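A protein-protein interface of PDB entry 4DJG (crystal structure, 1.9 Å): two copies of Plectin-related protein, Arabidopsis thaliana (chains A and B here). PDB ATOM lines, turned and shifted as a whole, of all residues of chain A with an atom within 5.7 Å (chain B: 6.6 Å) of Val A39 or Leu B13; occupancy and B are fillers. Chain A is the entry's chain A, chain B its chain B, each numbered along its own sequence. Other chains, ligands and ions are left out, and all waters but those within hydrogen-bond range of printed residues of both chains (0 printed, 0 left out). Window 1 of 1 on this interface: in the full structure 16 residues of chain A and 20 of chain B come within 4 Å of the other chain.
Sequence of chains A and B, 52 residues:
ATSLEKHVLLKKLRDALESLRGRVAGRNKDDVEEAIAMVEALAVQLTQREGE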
ATOM      1  N   LEU A  10     -21.623 -10.583  25.964  1.00  0.00           N
ATOM      2  CA  LEU A  10     -22.723  -9.919  26.668  1.00  0.00           C
ATOM      3  C   LEU A  10     -22.461  -9.738  28.169  1.00  0.00           C
ATOM      4  O   LEU A  10     -22.718  -8.663  28.735  1.00  0.00           O
ATOM      5  CB  LEU A  10     -24.054 -10.651  26.432  1.00  0.00           C
ATOM      6  CG  LEU A  10     -25.347  -9.941  26.864  1.00  0.00           C
ATOM      7  CD1 LEU A  10     -25.478  -8.534  26.283  1.00  0.00           C
ATOM      8  CD2 LEU A  10     -26.544 -10.787  26.476  1.00  0.00           C
ATOM      9  N   LEU A  13     -19.962  -6.970  28.703  1.00  0.00           N
ATOM     10  CA  LEU A  13     -20.595  -5.686  28.418  1.00  0.00           C
ATOM     11  C   LEU A  13     -21.427  -5.230  29.612  1.00  0.00           C
ATOM     12  O   LEU A  13     -21.389  -4.061  30.003  1.00  0.00           O
ATOM     13  CB  LEU A  13     -21.454  -5.757  27.148  1.00  0.00           C
ATOM     14  CG  LEU A  13     -22.276  -4.496  26.845  1.00  0.00           C
ATOM     15  CD1 LEU A  13     -21.400  -3.270  26.616  1.00  0.00           C
ATOM     16  CD2 LEU A  13     -23.165  -4.765  25.645  1.00  0.00           C
ATOM     17  N   ARG A  14     -22.182  -6.154  30.191  1.00  0.00           N
ATOM     18  CA  ARG A  14     -22.902  -5.857  31.417  1.00  0.00           C
ATOM     19  C   ARG A  14     -21.944  -5.356  32.504  1.00  0.00           C
ATOM     20  O   ARG A  14     -22.214  -4.338  33.153  1.00  0.00           O
ATOM     21  CB  ARG A  14     -23.692  -7.079  31.898  1.00  0.00           C
ATOM     22  CG  ARG A  14     -24.357  -6.873  33.252  1.00  0.00           C
ATOM     23  CD  ARG A  14     -25.473  -7.870  33.482  1.00  0.00           C
ATOM     24  NE  ARG A  14     -25.100  -9.272  33.732  1.00  0.00           N
ATOM     25  CZ  ARG A  14     -23.978  -9.734  34.289  1.00  0.00           C
ATOM     26  NH1 ARG A  14     -23.837 -11.047  34.455  1.00  0.00           N
ATOM     27  NH2 ARG A  14     -22.999  -8.925  34.684  1.00  0.00           N
ATOM     28  N   LEU A  17     -20.575  -1.849  31.745  1.00  0.00           N
ATOM     29  CA  LEU A  17     -21.569  -0.816  32.003  1.00  0.00           C
ATOM     30  C   LEU A  17     -21.790  -0.547  33.500  1.00  0.00           C
ATOM     31  O   LEU A  17     -21.878   0.611  33.928  1.00  0.00           O
ATOM     32  CB  LEU A  17     -22.892  -1.138  31.298  1.00  0.00           C
ATOM     33  CG  LEU A  17     -22.946  -1.197  29.754  1.00  0.00           C
ATOM     34  CD1 LEU A  17     -24.309  -1.686  29.284  1.00  0.00           C
ATOM     35  CD2 LEU A  17     -22.604   0.148  29.111  1.00  0.00           C
ATOM     36  N   GLU A  34     -29.818   3.334  31.115  1.00  0.00           N
ATOM     37  CA  GLU A  34     -30.586   2.938  29.922  1.00  0.00           C
ATOM     38  C   GLU A  34     -29.909   1.771  29.186  1.00  0.00           C
ATOM     39  O   GLU A  34     -30.545   0.743  28.935  1.00  0.00           O
ATOM     40  CB  GLU A  34     -30.848   4.156  29.019  1.00  0.00           C
ATOM     41  CG  GLU A  34     -31.520   3.895  27.668  1.00  0.00           C
ATOM     42  CD  GLU A  34     -32.942   3.337  27.741  1.00  0.00           C
ATOM     43  OE1 GLU A  34     -33.556   3.276  28.831  1.00  0.00           O
ATOM     44  OE2 GLU A  34     -33.467   2.943  26.677  1.00  0.00           O
ATOM     45  N   ALA A  35     -28.622   1.913  28.884  1.00  0.00           N
ATOM     46  CA  ALA A  35     -27.846   0.824  28.313  1.00  0.00           C
ATOM     47  C   ALA A  35     -27.912  -0.472  29.156  1.00  0.00           C
ATOM     48  O   ALA A  35     -28.093  -1.589  28.622  1.00  0.00           O
ATOM     49  CB  ALA A  35     -26.403   1.272  28.121  1.00  0.00           C
ATOM     50  N   ILE A  36     -27.765  -0.324  30.472  1.00  0.00           N
ATOM     51  CA  ILE A  36     -27.806  -1.477  31.383  1.00  0.00           C
ATOM     52  C   ILE A  36     -29.148  -2.207  31.271  1.00  0.00           C
ATOM     53  O   ILE A  36     -29.183  -3.441  31.148  1.00  0.00           O
ATOM     54  CB  ILE A  36     -27.508  -1.062  32.841  1.00  0.00           C
ATOM     55  CG1 ILE A  36     -26.021  -0.708  33.000  1.00  0.00           C
ATOM     56  CG2 ILE A  36     -27.922  -2.167  33.814  1.00  0.00           C
ATOM     57  CD1 ILE A  36     -25.653  -0.027  34.300  1.00  0.00           C
ATOM     58  N   ALA A  37     -30.244  -1.443  31.291  1.00  0.00           N
ATOM     59  CA  ALA A  37     -31.583  -2.007  31.136  1.00  0.00           C
ATOM     60  C   ALA A  37     -31.745  -2.754  29.798  1.00  0.00           C
ATOM     61  O   ALA A  37     -32.334  -3.850  29.762  1.00  0.00           O
ATOM     62  CB  ALA A  37     -32.636  -0.918  31.292  1.00  0.00           C
ATOM     63  N   MET A  38     -31.208  -2.180  28.715  1.00  0.00           N
ATOM     64  CA  MET A  38     -31.240  -2.838  27.390  1.00  0.00           C
ATOM     65  C   MET A  38     -30.486  -4.162  27.403  1.00  0.00           C
ATOM     66  O   MET A  38     -30.958  -5.160  26.850  1.00  0.00           O
ATOM     67  CB  MET A  38     -30.704  -1.929  26.268  1.00  0.00           C
ATOM     68  CG  MET A  38     -31.523  -0.672  25.981  1.00  0.00           C
ATOM     69  SD  MET A  38     -33.257  -0.959  25.569  1.00  0.00           S
ATOM     70  CE  MET A  38     -34.010  -0.975  27.182  1.00  0.00           C
ATOM     71  N   VAL A  39     -29.322  -4.168  28.047  1.00  0.00           N
ATOM     72  CA  VAL A  39     -28.501  -5.365  28.172  1.00  0.00           C
ATOM     73  C   VAL A  39     -29.196  -6.442  29.015  1.00  0.00           C
ATOM     74  O   VAL A  39     -29.164  -7.623  28.648  1.00  0.00           O
ATOM     75  CB  VAL A  39     -27.088  -5.010  28.697  1.00  0.00           C
ATOM     76  CG1 VAL A  39     -26.352  -6.240  29.242  1.00  0.00           C
ATOM     77  CG2 VAL A  39     -26.293  -4.377  27.572  1.00  0.00           C
ATOM     78  N   GLU A  40     -29.846  -6.036  30.108  1.00  0.00           N
ATOM     79  CA  GLU A  40     -30.613  -6.969  30.948  1.00  0.00           C
ATOM     80  C   GLU A  40     -31.768  -7.614  30.194  1.00  0.00           C
ATOM     81  O   GLU A  40     -32.010  -8.820  30.337  1.00  0.00           O
ATOM     82  CB  GLU A  40     -31.120  -6.290  32.218  1.00  0.00           C
ATOM     83  CG  GLU A  40     -30.019  -5.975  33.205  1.00  0.00           C
ATOM     84  CD  GLU A  40     -30.531  -5.634  34.590  1.00  0.00           C
ATOM     85  OE1 GLU A  40     -31.751  -5.741  34.825  1.00  0.00           O
ATOM     86  OE2 GLU A  40     -29.696  -5.267  35.448  1.00  0.00           O
ATOM     87  N   ALA A  41     -32.474  -6.820  29.392  1.00  0.00           N
ATOM     88  CA  ALA A  41     -33.527  -7.342  28.531  1.00  0.00           C
ATOM     89  C   ALA A  41     -32.979  -8.333  27.492  1.00  0.00           C
ATOM     90  O   ALA A  41     -33.540  -9.423  27.316  1.00  0.00           O
ATOM     91  CB  ALA A  41     -34.295  -6.211  27.872  1.00  0.00           C
ATOM     92  N   LEU A  42     -31.870  -7.975  26.839  1.00  0.00           N
ATOM     93  CA  LEU A  42     -31.225  -8.860  25.857  1.00  0.00           C
ATOM     94  C   LEU A  42     -30.691 -10.154  26.487  1.00  0.00           C
ATOM     95  O   LEU A  42     -30.824 -11.240  25.909  1.00  0.00           O
ATOM     96  CB  LEU A  42     -30.128  -8.106  25.086  1.00  0.00           C
ATOM     97  CG  LEU A  42     -30.585  -7.061  24.059  1.00  0.00           C
ATOM     98  CD1 LEU A  42     -29.505  -6.017  23.821  1.00  0.00           C
ATOM     99  CD2 LEU A  42     -31.006  -7.717  22.742  1.00  0.00           C
ATOM    100  N   ALA A  43     -30.122 -10.044  27.682  1.00  0.00           N
ATOM    101  CA  ALA A  43     -29.591 -11.197  28.421  1.00  0.00           C
ATOM    102  C   ALA A  43     -30.675 -12.211  28.802  1.00  0.00           C
ATOM    103  O   ALA A  43     -30.510 -13.430  28.620  1.00  0.00           O
ATOM    104  CB  ALA A  43     -28.850 -10.728  29.667  1.00  0.00           C
ATOM    105  N   VAL A  44     -31.771 -11.693  29.351  1.00  0.00           N
ATOM    106  CA  VAL A  44     -32.920 -12.499  29.758  1.00  0.00           C
ATOM    107  C   VAL A  44     -33.479 -13.330  28.593  1.00  0.00           C
ATOM    108  O   VAL A  44     -33.748 -14.530  28.749  1.00  0.00           O
ATOM    109  CB  VAL A  44     -34.006 -11.597  30.385  1.00  0.00           C
ATOM    110  CG1 VAL A  44     -35.365 -12.261  30.342  1.00  0.00           C
ATOM    111  CG2 VAL A  44     -33.622 -11.224  31.810  1.00  0.00           C
ATOM    112  N   VAL B   8     -34.741  -3.492  18.331  1.00  0.00           N
ATOM    113  CA  VAL B   8     -35.079  -2.233  18.997  1.00  0.00           C
ATOM    114  C   VAL B   8     -34.166  -2.040  20.214  1.00  0.00           C
ATOM    115  O   VAL B   8     -33.646  -0.934  20.455  1.00  0.00           O
ATOM    116  CB  VAL B   8     -36.584  -2.149  19.359  1.00  0.00           C
ATOM    117  CG1 VAL B   8     -36.845  -1.150  20.480  1.00  0.00           C
ATOM    118  CG2 VAL B   8     -37.402  -1.769  18.129  1.00  0.00           C
ATOM    119  N   LEU B   9     -33.954  -3.121  20.959  1.00  0.00           N
ATOM    120  CA  LEU B   9     -33.121  -3.063  22.155  1.00  0.00           C
ATOM    121  C   LEU B   9     -31.683  -2.714  21.796  1.00  0.00           C
ATOM    122  O   LEU B   9     -31.066  -1.890  22.464  1.00  0.00           O
ATOM    123  CB  LEU B   9     -33.190  -4.380  22.930  1.00  0.00           C
ATOM    124  CG  LEU B   9     -34.559  -4.792  23.491  1.00  0.00           C
ATOM    125  CD1 LEU B   9     -34.511  -6.213  24.033  1.00  0.00           C
ATOM    126  CD2 LEU B   9     -35.044  -3.809  24.553  1.00  0.00           C
ATOM    127  N   LEU B  10     -31.162  -3.331  20.732  1.00  0.00           N
ATOM    128  CA  LEU B  10     -29.786  -3.071  20.274  1.00  0.00           C
ATOM    129  C   LEU B  10     -29.583  -1.643  19.737  1.00  0.00           C
ATOM    130  O   LEU B  10     -28.530  -1.024  19.944  1.00  0.00           O
ATOM    131  CB  LEU B  10     -29.360  -4.110  19.224  1.00  0.00           C
ATOM    132  CG  LEU B  10     -29.135  -5.537  19.720  1.00  0.00           C
ATOM    133  CD1 LEU B  10     -29.276  -6.512  18.558  1.00  0.00           C
ATOM    134  CD2 LEU B  10     -27.795  -5.713  20.430  1.00  0.00           C
ATOM    135  N   LYS B  11     -30.601  -1.121  19.057  1.00  0.00           N
ATOM    136  CA  LYS B  11     -30.595   0.261  18.594  1.00  0.00           C
ATOM    137  C   LYS B  11     -30.583   1.274  19.763  1.00  0.00           C
ATOM    138  O   LYS B  11     -29.790   2.216  19.769  1.00  0.00           O
ATOM    139  CB  LYS B  11     -31.807   0.504  17.680  1.00  0.00           C
ATOM    140  CG  LYS B  11     -32.056   1.968  17.308  1.00  0.00           C
ATOM    141  CD  LYS B  11     -33.413   2.184  16.625  1.00  0.00           C
ATOM    142  CE  LYS B  11     -34.603   1.951  17.563  1.00  0.00           C
ATOM    143  NZ  LYS B  11     -35.000   3.141  18.377  1.00  0.00           N
ATOM    144  N   LYS B  12     -31.477   1.077  20.730  1.00  0.00           N
ATOM    145  CA  LYS B  12     -31.553   1.920  21.930  1.00  0.00           C
ATOM    146  C   LYS B  12     -30.228   1.876  22.710  1.00  0.00           C
ATOM    147  O   LYS B  12     -29.766   2.895  23.245  1.00  0.00           O
ATOM    148  CB  LYS B  12     -32.695   1.465  22.846  1.00  0.00           C
ATOM    149  CG  LYS B  12     -34.104   1.776  22.354  1.00  0.00           C
ATOM    150  CD  LYS B  12     -34.580   3.122  22.850  1.00  0.00           C
ATOM    151  CE  LYS B  12     -35.947   3.445  22.270  1.00  0.00           C
ATOM    152  NZ  LYS B  12     -36.449   4.708  22.866  1.00  0.00           N
ATOM    153  N   LEU B  13     -29.633   0.690  22.750  1.00  0.00           N
ATOM    154  CA  LEU B  13     -28.376   0.466  23.447  1.00  0.00           C
ATOM    155  C   LEU B  13     -27.270   1.268  22.765  1.00  0.00           C
ATOM    156  O   LEU B  13     -26.554   2.022  23.431  1.00  0.00           O
ATOM    157  CB  LEU B  13     -28.054  -1.040  23.488  1.00  0.00           C
ATOM    158  CG  LEU B  13     -26.718  -1.537  24.068  1.00  0.00           C
ATOM    159  CD1 LEU B  13     -26.505  -1.035  25.488  1.00  0.00           C
ATOM    160  CD2 LEU B  13     -26.624  -3.061  24.045  1.00  0.00           C
ATOM    161  N   ARG B  14     -27.156   1.129  21.443  1.00  0.00           N
ATOM    162  CA  ARG B  14     -26.181   1.898  20.666  1.00  0.00           C
ATOM    163  C   ARG B  14     -26.345   3.412  20.836  1.00  0.00           C
ATOM    164  O   ARG B  14     -25.357   4.122  21.028  1.00  0.00           O
ATOM    165  CB  ARG B  14     -26.252   1.528  19.174  1.00  0.00           C
ATOM    166  CG  ARG B  14     -25.517   2.507  18.263  1.00  0.00           C
ATOM    167  CD  ARG B  14     -26.080   2.546  16.843  1.00  0.00           C
ATOM    168  NE  ARG B  14     -25.419   1.575  15.976  1.00  0.00           N
ATOM    169  CZ  ARG B  14     -25.616   1.467  14.655  1.00  0.00           C
ATOM    170  NH1 ARG B  14     -26.470   2.274  14.031  1.00  0.00           N
ATOM    171  NH2 ARG B  14     -24.957   0.543  13.959  1.00  0.00           N
ATOM    172  N   ASP B  15     -27.587   3.893  20.736  1.00  0.00           N
ATOM    173  CA  ASP B  15     -27.889   5.326  20.819  1.00  0.00           C
ATOM    174  C   ASP B  15     -27.572   5.935  22.198  1.00  0.00           C
ATOM    175  O   ASP B  15     -27.101   7.075  22.294  1.00  0.00           O
ATOM    176  CB  ASP B  15     -29.357   5.580  20.469  1.00  0.00           C
ATOM    177  CG  ASP B  15     -29.653   5.397  18.983  1.00  0.00           C
ATOM    178  OD1 ASP B  15     -28.749   5.045  18.201  1.00  0.00           O
ATOM    179  OD2 ASP B  15     -30.821   5.588  18.609  1.00  0.00           O
ATOM    180  N   ALA B  16     -27.848   5.178  23.256  1.00  0.00           N
ATOM    181  CA  ALA B  16     -27.564   5.625  24.612  1.00  0.00           C
ATOM    182  C   ALA B  16     -26.056   5.864  24.803  1.00  0.00           C
ATOM    183  O   ALA B  16     -25.626   6.912  25.301  1.00  0.00           O
ATOM    184  CB  ALA B  16     -28.076   4.600  25.612  1.00  0.00           C
ATOM    185  N   LEU B  17     -25.257   4.885  24.392  1.00  0.00           N
ATOM    186  CA  LEU B  17     -23.800   4.956  24.501  1.00  0.00           C
ATOM    187  C   LEU B  17     -23.185   6.004  23.590  1.00  0.00           C
ATOM    188  O   LEU B  17     -22.252   6.686  23.985  1.00  0.00           O
ATOM    189  CB  LEU B  17     -23.174   3.594  24.228  1.00  0.00           C
ATOM    190  CG  LEU B  17     -23.507   2.526  25.274  1.00  0.00           C
ATOM    191  CD1 LEU B  17     -22.715   1.274  24.950  1.00  0.00           C
ATOM    192  CD2 LEU B  17     -23.181   3.013  26.686  1.00  0.00           C
ATOM    193  N   GLU B  18     -23.719   6.143  22.383  1.00  0.00           N
ATOM    194  CA  GLU B  18     -23.263   7.190  21.473  1.00  0.00           C
ATOM    195  C   GLU B  18     -23.395   8.611  22.059  1.00  0.00           C
ATOM    196  O   GLU B  18     -22.529   9.466  21.826  1.00  0.00           O
ATOM    197  CB  GLU B  18     -24.000   7.059  20.130  1.00  0.00           C
ATOM    198  CG  GLU B  18     -23.546   8.027  19.055  1.00  0.00           C
ATOM    199  CD  GLU B  18     -22.106   7.805  18.627  1.00  0.00           C
ATOM    200  OE1 GLU B  18     -21.614   6.657  18.697  1.00  0.00           O
ATOM    201  OE2 GLU B  18     -21.467   8.793  18.202  1.00  0.00           O
ATOM    202  N   VAL B  39     -21.014  -3.369  21.766  1.00  0.00           N
ATOM    203  CA  VAL B  39     -22.396  -3.315  21.288  1.00  0.00           C
ATOM    204  C   VAL B  39     -22.490  -3.596  19.777  1.00  0.00           C
ATOM    205  O   VAL B  39     -23.360  -4.353  19.333  1.00  0.00           O
ATOM    206  CB  VAL B  39     -23.053  -1.968  21.649  1.00  0.00           C
ATOM    207  CG1 VAL B  39     -24.400  -1.818  20.946  1.00  0.00           C
ATOM    208  CG2 VAL B  39     -23.245  -1.887  23.160  1.00  0.00           C
ATOM    209  N   LEU B  42     -21.935  -7.233  19.182  1.00  0.00           N
ATOM    210  CA  LEU B  42     -23.132  -7.934  19.612  1.00  0.00           C
ATOM    211  C   LEU B  42     -24.232  -7.832  18.550  1.00  0.00           C
ATOM    212  O   LEU B  42     -24.945  -8.805  18.283  1.00  0.00           O
ATOM    213  CB  LEU B  42     -23.598  -7.322  20.936  1.00  0.00           C
ATOM    214  CG  LEU B  42     -24.241  -8.096  22.084  1.00  0.00           C
ATOM    215  CD1 LEU B  42     -23.680  -9.498  22.277  1.00  0.00           C
ATOM    216  CD2 LEU B  42     -24.039  -7.253  23.332  1.00  0.00           C
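Leu A10 touches Leu B42, and with the chains exchanged Leu A42 touches Leu B10. Leu A13 touches Val B39, and with the chains exchanged Val A39 touches Leu B13. Leu A13 touches Leu B42, but with the chains exchanged Leu A42 does not touch Leu B13 (4.1 Å). Leu B17 touches its own counterpart, Leu A17. 6 positions are printed for both chains. Of the 14 pairs that touch across the chains among the printed residues, 5 have their exchanged pair printed and touching as well.
Leu A10 touches Leu B42. Val B39 touches Leu A13. Glu A34 touches Lys B12 (OE2 to CD, 3.99 Å). Ala A35 touches Leu B17. CD2 of Leu B9 touches SD of Met A38, 3.5 Å away. Leu B13 touches Met A38 (CB to CB, 3.9 Å). Val A39 touches Leu B13 (CG2 to CD2, 3.8 Å). Leu B9 touches Ala A41. Leu A42 touches Leu B9. Leu A42 touches Leu B10.
Printed residues of chain B within 4 Å of Leu A10: Leu B42 (3.5 Å). Of the printed residues of chain B, Ala A35 touches Leu B13 and Leu B17. Ala A37 touches none of the printed residues of chain B. Printed residues of chain B within 4 Å of Met A38: Leu B9 (3.5 Å), Lys B12 (3.7 Å) and Leu B13 (3.9 Å). Of the printed residues of chain B, Val A39 touches Leu B13 (3.8 Å). Val A44 touches none of the printed residues of chain B. Printed residues of chain A within 4 Å of Lys B12: Glu A34 (3.99 Å) and Met A38 (3.7 Å). Leu B13 touches three residues of chain A. Of the printed residues of chain A, Leu B42 touches Leu A10 (3.5 Å) and Leu A13 (3.5 Å). The nearest residue of chain A that does not touch Leu B13 is Leu A42 (4.1 Å). The nearest printed residue of chain B that does not touch Leu A17 is Leu B13 (4.4 Å).
Hydrophobic or aromatic side chains of chain A within 4 Å of the printed part of chain B: Leu A10, Leu A13, Leu A17, Ala A35, Met A38, Val A39, Ala A41 and Leu A42. Among the printed residues, 14 pairs touch across the chains. Among the printed residues, no Asp or Glu carboxylate lies within 4 Å of a Lys or Arg side-chain nitrogen of the other chain.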
